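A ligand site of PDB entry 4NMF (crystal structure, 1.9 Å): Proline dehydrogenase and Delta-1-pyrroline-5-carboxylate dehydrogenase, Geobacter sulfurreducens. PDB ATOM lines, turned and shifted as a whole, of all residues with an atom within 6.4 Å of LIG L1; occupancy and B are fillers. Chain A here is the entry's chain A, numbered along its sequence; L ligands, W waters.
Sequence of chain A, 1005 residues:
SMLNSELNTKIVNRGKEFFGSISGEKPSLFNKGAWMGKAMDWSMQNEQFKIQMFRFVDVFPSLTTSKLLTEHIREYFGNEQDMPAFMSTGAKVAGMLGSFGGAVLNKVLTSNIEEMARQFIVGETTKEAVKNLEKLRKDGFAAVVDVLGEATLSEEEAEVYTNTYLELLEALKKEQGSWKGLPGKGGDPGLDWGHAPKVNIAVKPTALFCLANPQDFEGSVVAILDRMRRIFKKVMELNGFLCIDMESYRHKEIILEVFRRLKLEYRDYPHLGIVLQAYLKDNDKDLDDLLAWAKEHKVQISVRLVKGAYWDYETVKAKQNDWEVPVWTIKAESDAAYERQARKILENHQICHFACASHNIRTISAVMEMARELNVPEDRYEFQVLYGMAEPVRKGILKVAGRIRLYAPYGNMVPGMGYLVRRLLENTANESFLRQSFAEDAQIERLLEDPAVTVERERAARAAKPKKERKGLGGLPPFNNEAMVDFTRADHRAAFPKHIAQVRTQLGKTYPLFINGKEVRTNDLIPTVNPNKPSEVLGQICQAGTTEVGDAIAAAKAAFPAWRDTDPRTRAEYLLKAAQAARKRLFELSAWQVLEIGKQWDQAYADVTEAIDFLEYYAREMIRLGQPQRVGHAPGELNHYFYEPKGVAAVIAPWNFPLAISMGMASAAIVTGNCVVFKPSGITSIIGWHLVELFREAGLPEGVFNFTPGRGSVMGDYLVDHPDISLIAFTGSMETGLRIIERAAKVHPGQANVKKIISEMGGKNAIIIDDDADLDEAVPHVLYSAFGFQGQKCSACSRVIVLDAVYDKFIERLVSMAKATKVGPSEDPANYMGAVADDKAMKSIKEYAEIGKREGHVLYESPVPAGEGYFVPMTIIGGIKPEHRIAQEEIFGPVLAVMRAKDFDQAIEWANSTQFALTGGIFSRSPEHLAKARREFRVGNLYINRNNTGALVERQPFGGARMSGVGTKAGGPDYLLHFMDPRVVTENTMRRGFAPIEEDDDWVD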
ATOM      1  N   ASP A 146     -14.891  29.911 -20.765  1.00  0.00           N
ATOM      2  CA  ASP A 146     -16.184  29.237 -20.736  1.00  0.00           C
ATOM      3  C   ASP A 146     -16.346  28.493 -19.423  1.00  0.00           C
ATOM      4  O   ASP A 146     -15.371  27.989 -18.854  1.00  0.00           O
ATOM      5  CB  ASP A 146     -16.294  28.276 -21.914  1.00  0.00           C
ATOM      6  CG  ASP A 146     -17.454  27.321 -21.777  1.00  0.00           C
ATOM      7  OD1 ASP A 146     -18.610  27.800 -21.772  1.00  0.00           O
ATOM      8  OD2 ASP A 146     -17.218  26.095 -21.703  1.00  0.00           O
ATOM      9  N   LEU A 148     -17.721  25.347 -17.499  1.00  0.00           N
ATOM     10  CA  LEU A 148     -18.203  23.969 -17.582  1.00  0.00           C
ATOM     11  C   LEU A 148     -19.392  23.767 -16.655  1.00  0.00           C
ATOM     12  O   LEU A 148     -19.371  24.234 -15.521  1.00  0.00           O
ATOM     13  CB  LEU A 148     -17.108  22.985 -17.148  1.00  0.00           C
ATOM     14  CG  LEU A 148     -15.894  22.673 -18.007  1.00  0.00           C
ATOM     15  CD1 LEU A 148     -14.938  21.790 -17.223  1.00  0.00           C
ATOM     16  CD2 LEU A 148     -16.302  21.981 -19.293  1.00  0.00           C
ATOM     17  N   LYS A 204     -23.139  29.299 -23.147  1.00  0.00           N
ATOM     18  CA  LYS A 204     -23.982  28.316 -23.840  1.00  0.00           C
ATOM     19  C   LYS A 204     -25.418  28.703 -23.560  1.00  0.00           C
ATOM     20  O   LYS A 204     -25.888  28.622 -22.387  1.00  0.00           O
ATOM     21  CB  LYS A 204     -23.720  26.880 -23.398  1.00  0.00           C
ATOM     22  CG  LYS A 204     -22.320  26.285 -23.459  1.00  0.00           C
ATOM     23  CD  LYS A 204     -21.474  26.535 -24.672  1.00  0.00           C
ATOM     24  CE  LYS A 204     -20.789  25.374 -25.380  1.00  0.00           C
ATOM     25  NZ  LYS A 204     -19.405  25.562 -25.805  1.00  0.00           N
ATOM     26  N   ASP A 245     -22.427  31.014 -27.859  1.00  0.00           N
ATOM     27  CA  ASP A 245     -22.095  29.759 -28.515  1.00  0.00           C
ATOM     28  C   ASP A 245     -23.321  29.165 -29.196  1.00  0.00           C
ATOM     29  O   ASP A 245     -24.449  29.499 -28.856  1.00  0.00           O
ATOM     30  CB  ASP A 245     -21.494  28.743 -27.544  1.00  0.00           C
ATOM     31  CG  ASP A 245     -20.091  29.144 -27.040  1.00  0.00           C
ATOM     32  OD1 ASP A 245     -19.377  29.889 -27.731  1.00  0.00           O
ATOM     33  OD2 ASP A 245     -19.692  28.680 -25.950  1.00  0.00           O
ATOM     34  N   MET A 246     -23.095  28.291 -30.177  1.00  0.00           N
ATOM     35  CA  MET A 246     -24.213  27.683 -30.894  1.00  0.00           C
ATOM     36  C   MET A 246     -24.302  26.222 -30.504  1.00  0.00           C
ATOM     37  O   MET A 246     -23.286  25.512 -30.467  1.00  0.00           O
ATOM     38  CB  MET A 246     -24.003  27.812 -32.400  1.00  0.00           C
ATOM     39  CG  MET A 246     -25.143  27.229 -33.229  1.00  0.00           C
ATOM     40  SD  MET A 246     -26.747  27.993 -32.849  1.00  0.00           S
ATOM     41  CE  MET A 246     -26.536  29.595 -33.648  1.00  0.00           C
ATOM     42  N   ALA A 309     -20.248  20.778 -33.792  1.00  0.00           N
ATOM     43  CA  ALA A 309     -19.881  19.784 -32.771  1.00  0.00           C
ATOM     44  C   ALA A 309     -20.828  18.605 -32.603  1.00  0.00           C
ATOM     45  O   ALA A 309     -20.539  17.703 -31.816  1.00  0.00           O
ATOM     46  CB  ALA A 309     -19.694  20.459 -31.409  1.00  0.00           C
ATOM     47  N   TYR A 310     -21.956  18.608 -33.307  1.00  0.00           N
ATOM     48  CA  TYR A 310     -22.977  17.606 -33.006  1.00  0.00           C
ATOM     49  C   TYR A 310     -23.321  16.716 -34.192  1.00  0.00           C
ATOM     50  O   TYR A 310     -24.467  16.240 -34.311  1.00  0.00           O
ATOM     51  CB  TYR A 310     -24.250  18.303 -32.514  1.00  0.00           C
ATOM     52  CG  TYR A 310     -24.045  19.325 -31.397  1.00  0.00           C
ATOM     53  CD1 TYR A 310     -23.714  20.648 -31.684  1.00  0.00           C
ATOM     54  CD2 TYR A 310     -24.234  18.972 -30.072  1.00  0.00           C
ATOM     55  CE1 TYR A 310     -23.534  21.593 -30.644  1.00  0.00           C
ATOM     56  CE2 TYR A 310     -24.059  19.885 -29.046  1.00  0.00           C
ATOM     57  CZ  TYR A 310     -23.717  21.190 -29.337  1.00  0.00           C
ATOM     58  OH  TYR A 310     -23.567  22.074 -28.293  1.00  0.00           O
ATOM     59  N   LEU A 386      -9.274  25.182 -29.435  1.00  0.00           N
ATOM     60  CA  LEU A 386      -9.621  24.709 -28.099  1.00  0.00           C
ATOM     61  C   LEU A 386      -8.355  24.442 -27.298  1.00  0.00           C
ATOM     62  O   LEU A 386      -7.416  23.810 -27.790  1.00  0.00           O
ATOM     63  CB  LEU A 386     -10.471  23.437 -28.178  1.00  0.00           C
ATOM     64  CG  LEU A 386     -11.802  23.496 -28.913  1.00  0.00           C
ATOM     65  CD1 LEU A 386     -12.514  22.131 -28.839  1.00  0.00           C
ATOM     66  CD2 LEU A 386     -12.687  24.583 -28.362  1.00  0.00           C
ATOM     67  N   TYR A 407      -9.815  28.846 -26.537  1.00  0.00           N
ATOM     68  CA  TYR A 407     -11.100  28.646 -25.896  1.00  0.00           C
ATOM     69  C   TYR A 407     -10.856  27.812 -24.639  1.00  0.00           C
ATOM     70  O   TYR A 407     -10.510  26.634 -24.718  1.00  0.00           O
ATOM     71  CB  TYR A 407     -12.082  27.950 -26.828  1.00  0.00           C
ATOM     72  CG  TYR A 407     -13.501  27.962 -26.325  1.00  0.00           C
ATOM     73  CD1 TYR A 407     -13.899  27.090 -25.313  1.00  0.00           C
ATOM     74  CD2 TYR A 407     -14.448  28.823 -26.865  1.00  0.00           C
ATOM     75  CE1 TYR A 407     -15.190  27.101 -24.854  1.00  0.00           C
ATOM     76  CE2 TYR A 407     -15.755  28.829 -26.403  1.00  0.00           C
ATOM     77  CZ  TYR A 407     -16.113  27.961 -25.400  1.00  0.00           C
ATOM     78  OH  TYR A 407     -17.396  27.939 -24.910  1.00  0.00           O
ATOM     79  N   PRO A 409     -12.100  26.338 -21.173  1.00  0.00           N
ATOM     80  CA  PRO A 409     -13.168  26.018 -20.221  1.00  0.00           C
ATOM     81  C   PRO A 409     -12.578  25.697 -18.852  1.00  0.00           C
ATOM     82  O   PRO A 409     -11.409  25.309 -18.747  1.00  0.00           O
ATOM     83  CB  PRO A 409     -13.857  24.803 -20.855  1.00  0.00           C
ATOM     84  CG  PRO A 409     -12.780  24.129 -21.660  1.00  0.00           C
ATOM     85  CD  PRO A 409     -11.767  25.205 -22.045  1.00  0.00           C
ATOM     86  N   GLY A 418     -17.270  14.631 -19.205  1.00  0.00           N
ATOM     87  CA  GLY A 418     -18.132  14.564 -20.367  1.00  0.00           C
ATOM     88  C   GLY A 418     -17.516  15.324 -21.522  1.00  0.00           C
ATOM     89  O   GLY A 418     -17.630  14.930 -22.693  1.00  0.00           O
ATOM     90  N   TYR A 419     -16.845  16.429 -21.207  1.00  0.00           N
ATOM     91  CA  TYR A 419     -16.164  17.223 -22.211  1.00  0.00           C
ATOM     92  C   TYR A 419     -14.976  16.440 -22.752  1.00  0.00           C
ATOM     93  O   TYR A 419     -14.738  16.422 -23.965  1.00  0.00           O
ATOM     94  CB  TYR A 419     -15.717  18.550 -21.605  1.00  0.00           C
ATOM     95  CG  TYR A 419     -14.942  19.457 -22.534  1.00  0.00           C
ATOM     96  CD1 TYR A 419     -15.522  19.967 -23.697  1.00  0.00           C
ATOM     97  CD2 TYR A 419     -13.649  19.845 -22.231  1.00  0.00           C
ATOM     98  CE1 TYR A 419     -14.793  20.820 -24.543  1.00  0.00           C
ATOM     99  CE2 TYR A 419     -12.927  20.689 -23.055  1.00  0.00           C
ATOM    100  CZ  TYR A 419     -13.499  21.181 -24.205  1.00  0.00           C
ATOM    101  OH  TYR A 419     -12.767  22.021 -25.009  1.00  0.00           O
ATOM    102  N   ARG A 422     -16.024  13.959 -25.385  1.00  0.00           N
ATOM    103  CA  ARG A 422     -16.287  14.594 -26.673  1.00  0.00           C
ATOM    104  C   ARG A 422     -15.005  15.010 -27.405  1.00  0.00           C
ATOM    105  O   ARG A 422     -14.907  14.861 -28.633  1.00  0.00           O
ATOM    106  CB  ARG A 422     -17.295  15.737 -26.495  1.00  0.00           C
ATOM    107  CG  ARG A 422     -18.532  15.209 -25.754  1.00  0.00           C
ATOM    108  CD  ARG A 422     -19.719  16.149 -25.808  1.00  0.00           C
ATOM    109  NE  ARG A 422     -19.892  16.674 -27.154  1.00  0.00           N
ATOM    110  CZ  ARG A 422     -20.954  16.450 -27.901  1.00  0.00           C
ATOM    111  NH1 ARG A 422     -21.027  16.982 -29.120  1.00  0.00           N
ATOM    112  NH2 ARG A 422     -21.965  15.717 -27.445  1.00  0.00           N
ATOM    113  N   ARG A 423     -14.004  15.474 -26.651  1.00  0.00           N
ATOM    114  CA  ARG A 423     -12.697  15.794 -27.226  1.00  0.00           C
ATOM    115  C   ARG A 423     -12.010  14.545 -27.799  1.00  0.00           C
ATOM    116  O   ARG A 423     -11.424  14.598 -28.888  1.00  0.00           O
ATOM    117  CB  ARG A 423     -11.767  16.415 -26.171  1.00  0.00           C
ATOM    118  CG  ARG A 423     -12.130  17.836 -25.702  1.00  0.00           C
ATOM    119  CD  ARG A 423     -12.302  18.807 -26.859  1.00  0.00           C
ATOM    120  NE  ARG A 423     -13.706  18.928 -27.249  1.00  0.00           N
ATOM    121  CZ  ARG A 423     -14.140  18.974 -28.506  1.00  0.00           C
ATOM    122  NH1 ARG A 423     -15.436  19.082 -28.755  1.00  0.00           N
ATOM    123  NH2 ARG A 423     -13.281  18.935 -29.520  1.00  0.00           N
HETATM  124  O1  LIG L   1     -18.649  18.635 -27.890  1.00  0.00           O
HETATM  125  S1  LIG L   1     -18.430  19.586 -26.818  1.00  0.00           S
HETATM  126  O2  LIG L   1     -18.686  18.938 -25.548  1.00  0.00           O
HETATM  127  O3  LIG L   1     -16.993  19.765 -26.836  1.00  0.00           O
HETATM  128  C1  LIG L   1     -19.400  21.057 -26.965  1.00  0.00           C
HETATM  129  C2  LIG L   1     -20.842  20.711 -27.151  1.00  0.00           C
HETATM  130  C3  LIG L   1     -18.901  21.885 -28.120  1.00  0.00           C
HETATM  131  C4  LIG L   1     -17.537  22.405 -27.824  1.00  0.00           C
HETATM  132  O4  LIG L   1     -16.586  22.460 -28.811  1.00  0.00           O
HETATM  133  C5  LIG L   1     -17.189  22.840 -26.448  1.00  0.00           C
HETATM  134  C6  LIG L   1     -15.946  23.602 -26.215  1.00  0.00           C
HETATM  135  C7  LIG L   1     -15.630  23.994 -24.907  1.00  0.00           C
HETATM  136  C8  LIG L   1     -16.484  23.685 -23.832  1.00  0.00           C
HETATM  137  C9  LIG L   1     -17.660  22.974 -24.043  1.00  0.00           C
HETATM  138  C10 LIG L   1     -17.999  22.549 -25.417  1.00  0.00           C
HETATM  139  C11 LIG L   1     -19.237  21.766 -25.661  1.00  0.00           C
HETATM  140  O5  LIG L   1     -20.197  21.671 -24.682  1.00  0.00           O
HETATM  141  P1  LG2 L   2     -11.707  19.006 -38.944  1.00  0.00           P
HETATM  142  O1  LG2 L   2     -11.023  19.582 -40.211  1.00  0.00           O
HETATM  143  O2  LG2 L   2     -11.306  17.676 -38.546  1.00  0.00           O
HETATM  144  O3  LG2 L   2     -13.181  18.804 -39.023  1.00  0.00           O
HETATM  145  C1  LG2 L   2     -13.987  18.058 -38.116  1.00  0.00           C
HETATM  146  C2  LG2 L   2     -15.464  18.400 -38.359  1.00  0.00           C
HETATM  147  O4  LG2 L   2     -15.958  17.943 -39.601  1.00  0.00           O
HETATM  148  C3  LG2 L   2     -16.413  17.815 -37.361  1.00  0.00           C
HETATM  149  O5  LG2 L   2     -16.419  18.477 -36.154  1.00  0.00           O
HETATM  150  C4  LG2 L   2     -17.701  17.955 -38.063  1.00  0.00           C
HETATM  151  O6  LG2 L   2     -18.221  19.226 -37.902  1.00  0.00           O
HETATM  152  C5  LG2 L   2     -17.338  17.720 -39.483  1.00  0.00           C
HETATM  153  N1  LG2 L   2     -17.640  16.370 -39.923  1.00  0.00           N
HETATM  154  C6  LG2 L   2     -17.197  15.160 -39.408  1.00  0.00           C
HETATM  155  N2  LG2 L   2     -17.710  14.154 -40.137  1.00  0.00           N
HETATM  156  C7  LG2 L   2     -18.512  14.688 -41.140  1.00  0.00           C
HETATM  157  C8  LG2 L   2     -19.262  14.137 -42.156  1.00  0.00           C
HETATM  158  N3  LG2 L   2     -19.312  12.698 -42.312  1.00  0.00           N
HETATM  159  N4  LG2 L   2     -19.946  14.928 -43.000  1.00  0.00           N
HETATM  160  C9  LG2 L   2     -19.915  16.294 -42.873  1.00  0.00           C
HETATM  161  N5  LG2 L   2     -19.179  16.883 -41.884  1.00  0.00           N
HETATM  162  C10 LG2 L   2     -18.481  16.113 -41.018  1.00  0.00           C
HETATM  163  N6  LG2 L   2     -18.965  23.574 -32.321  1.00  0.00           N
HETATM  164  C11 LG2 L   2     -20.338  23.989 -32.310  1.00  0.00           C
HETATM  165  O7  LG2 L   2     -21.255  23.242 -33.010  1.00  0.00           O
HETATM  166  N7  LG2 L   2     -20.736  25.138 -31.605  1.00  0.00           N
HETATM  167  C12 LG2 L   2     -19.802  25.898 -30.895  1.00  0.00           C
HETATM  168  O8  LG2 L   2     -20.188  27.021 -30.206  1.00  0.00           O
HETATM  169  C13 LG2 L   2     -18.379  25.462 -30.890  1.00  0.00           C
HETATM  170  N8  LG2 L   2     -17.394  26.167 -30.099  1.00  0.00           N
HETATM  171  C14 LG2 L   2     -16.029  26.081 -30.574  1.00  0.00           C
HETATM  172  C15 LG2 L   2     -15.078  27.175 -30.228  1.00  0.00           C
HETATM  173  C16 LG2 L   2     -13.753  27.085 -30.693  1.00  0.00           C
HETATM  174  C17 LG2 L   2     -12.775  28.186 -30.359  1.00  0.00           C
HETATM  175  C18 LG2 L   2     -13.345  25.964 -31.484  1.00  0.00           C
HETATM  176  C19 LG2 L   2     -11.928  25.869 -32.000  1.00  0.00           C
HETATM  177  C20 LG2 L   2     -14.262  24.925 -31.822  1.00  0.00           C
HETATM  178  C21 LG2 L   2     -15.654  25.011 -31.324  1.00  0.00           C
HETATM  179  N9  LG2 L   2     -16.621  23.965 -31.643  1.00  0.00           N
HETATM  180  C22 LG2 L   2     -18.000  24.344 -31.575  1.00  0.00           C
HETATM  181  C23 LG2 L   2     -16.248  22.659 -32.238  1.00  0.00           C
HETATM  182  C24 LG2 L   2     -16.155  22.731 -33.747  1.00  0.00           C
HETATM  183  O9  LG2 L   2     -17.428  22.824 -34.298  1.00  0.00           O
HETATM  184  C25 LG2 L   2     -15.456  21.519 -34.370  1.00  0.00           C
HETATM  185  O10 LG2 L   2     -16.100  20.386 -33.894  1.00  0.00           O
HETATM  186  C26 LG2 L   2     -13.962  21.368 -34.091  1.00  0.00           C
HETATM  187  O11 LG2 L   2     -13.320  22.601 -34.022  1.00  0.00           O
HETATM  188  C27 LG2 L   2     -13.249  20.437 -35.085  1.00  0.00           C
HETATM  189  O12 LG2 L   2     -13.227  20.925 -36.414  1.00  0.00           O
HETATM  190  P2  LG2 L   2     -11.867  21.161 -37.227  1.00  0.00           P
HETATM  191  O13 LG2 L   2     -11.853  22.262 -38.342  1.00  0.00           O
HETATM  192  O14 LG2 L   2     -10.858  21.325 -36.020  1.00  0.00           O
HETATM  193  O15 LG2 L   2     -11.437  19.631 -37.612  1.00  0.00           O
HETATM  194  C28 LG2 L   2     -18.010  26.016 -27.795  1.00  0.00           C
HETATM  195  C29 LG2 L   2     -17.656  25.560 -29.001  1.00  0.00           C
HETATM  196  C30 LG2 L   2     -19.240  25.391 -27.125  1.00  0.00           C
HETATM  197  O   HOH W   1     -17.884  17.528 -30.554  1.00  0.00           O
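Asp 146 touches LIG L1 (OD2 to C8, 3.3 Å).
Lys 204 touches LIG L1.
CB of Ala 309 touches C3 of LIG L1, 3.7 Å away.
OH of Tyr 310 touches C2 of LIG L1, 3.3 Å away.
Tyr 407 touches LIG L1.
Tyr 419 touches LIG L1 (CE1 to C7, 3.3 Å).
Hydrophobic or aromatic side chains that line LIG L1: Ala 309, Tyr 310, Tyr 407 and Tyr 419.
Eight residues have an atom within 4 Å of LIG L1: Asp 146, Lys 204, Ala 309, Tyr 310, Tyr 407, Tyr 419, Arg 422 and Arg 423.
The nearest printed residue that does not touch LIG L1 is Leu 386 (4.02 Å).
The guanidinium group of Arg 422 lies within hydrogen-bond range of the backbone carbonyl oxygen of Ala 309 (2.8 Å).
OD1 of Asp 146 sits close to OH of Tyr 407, 3.4 Å away.
OH of Tyr 407 lies within hydrogen-bond range of NZ of Lys 204, 3.2 Å away.
OH of Tyr 407 is in hydrogen-bond range of OD2 of Asp 245.
OD2 of Asp 245 lies within salt-bridge range of NZ of Lys 204 (3.1 Å).
NE of Arg 422 lies within salt-bridge range of O1 of LIG L1.
An oxygen (O3) of LIG L1 lies within salt-bridge range of the guanidinium group (NH1) of Arg 423.
The side-chain amino group of Lys 204 is bonded to a carbon (C30) of LG2 L2 (1.3 Å).
O7 of LG2 L2 is in hydrogen-bond range of N of Ala 309, at 2.8 Å.
N of Met 246 lies within hydrogen-bond range of O8 of LG2 L2, at 3.2 Å.
The backbone carbonyl oxygen (O) of Met 246 sits at hydrogen-bond distance from a nitrogen (N7) of LG2 L2, 2.8 Å away.
Water W1 lies within hydrogen-bond range of O of Ala 309 (2.9 Å), O1 of LIG L1 (3.0 Å), NH1 of Arg 423 (3.4 Å) and NH1 of Arg 422 (3.5 Å).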
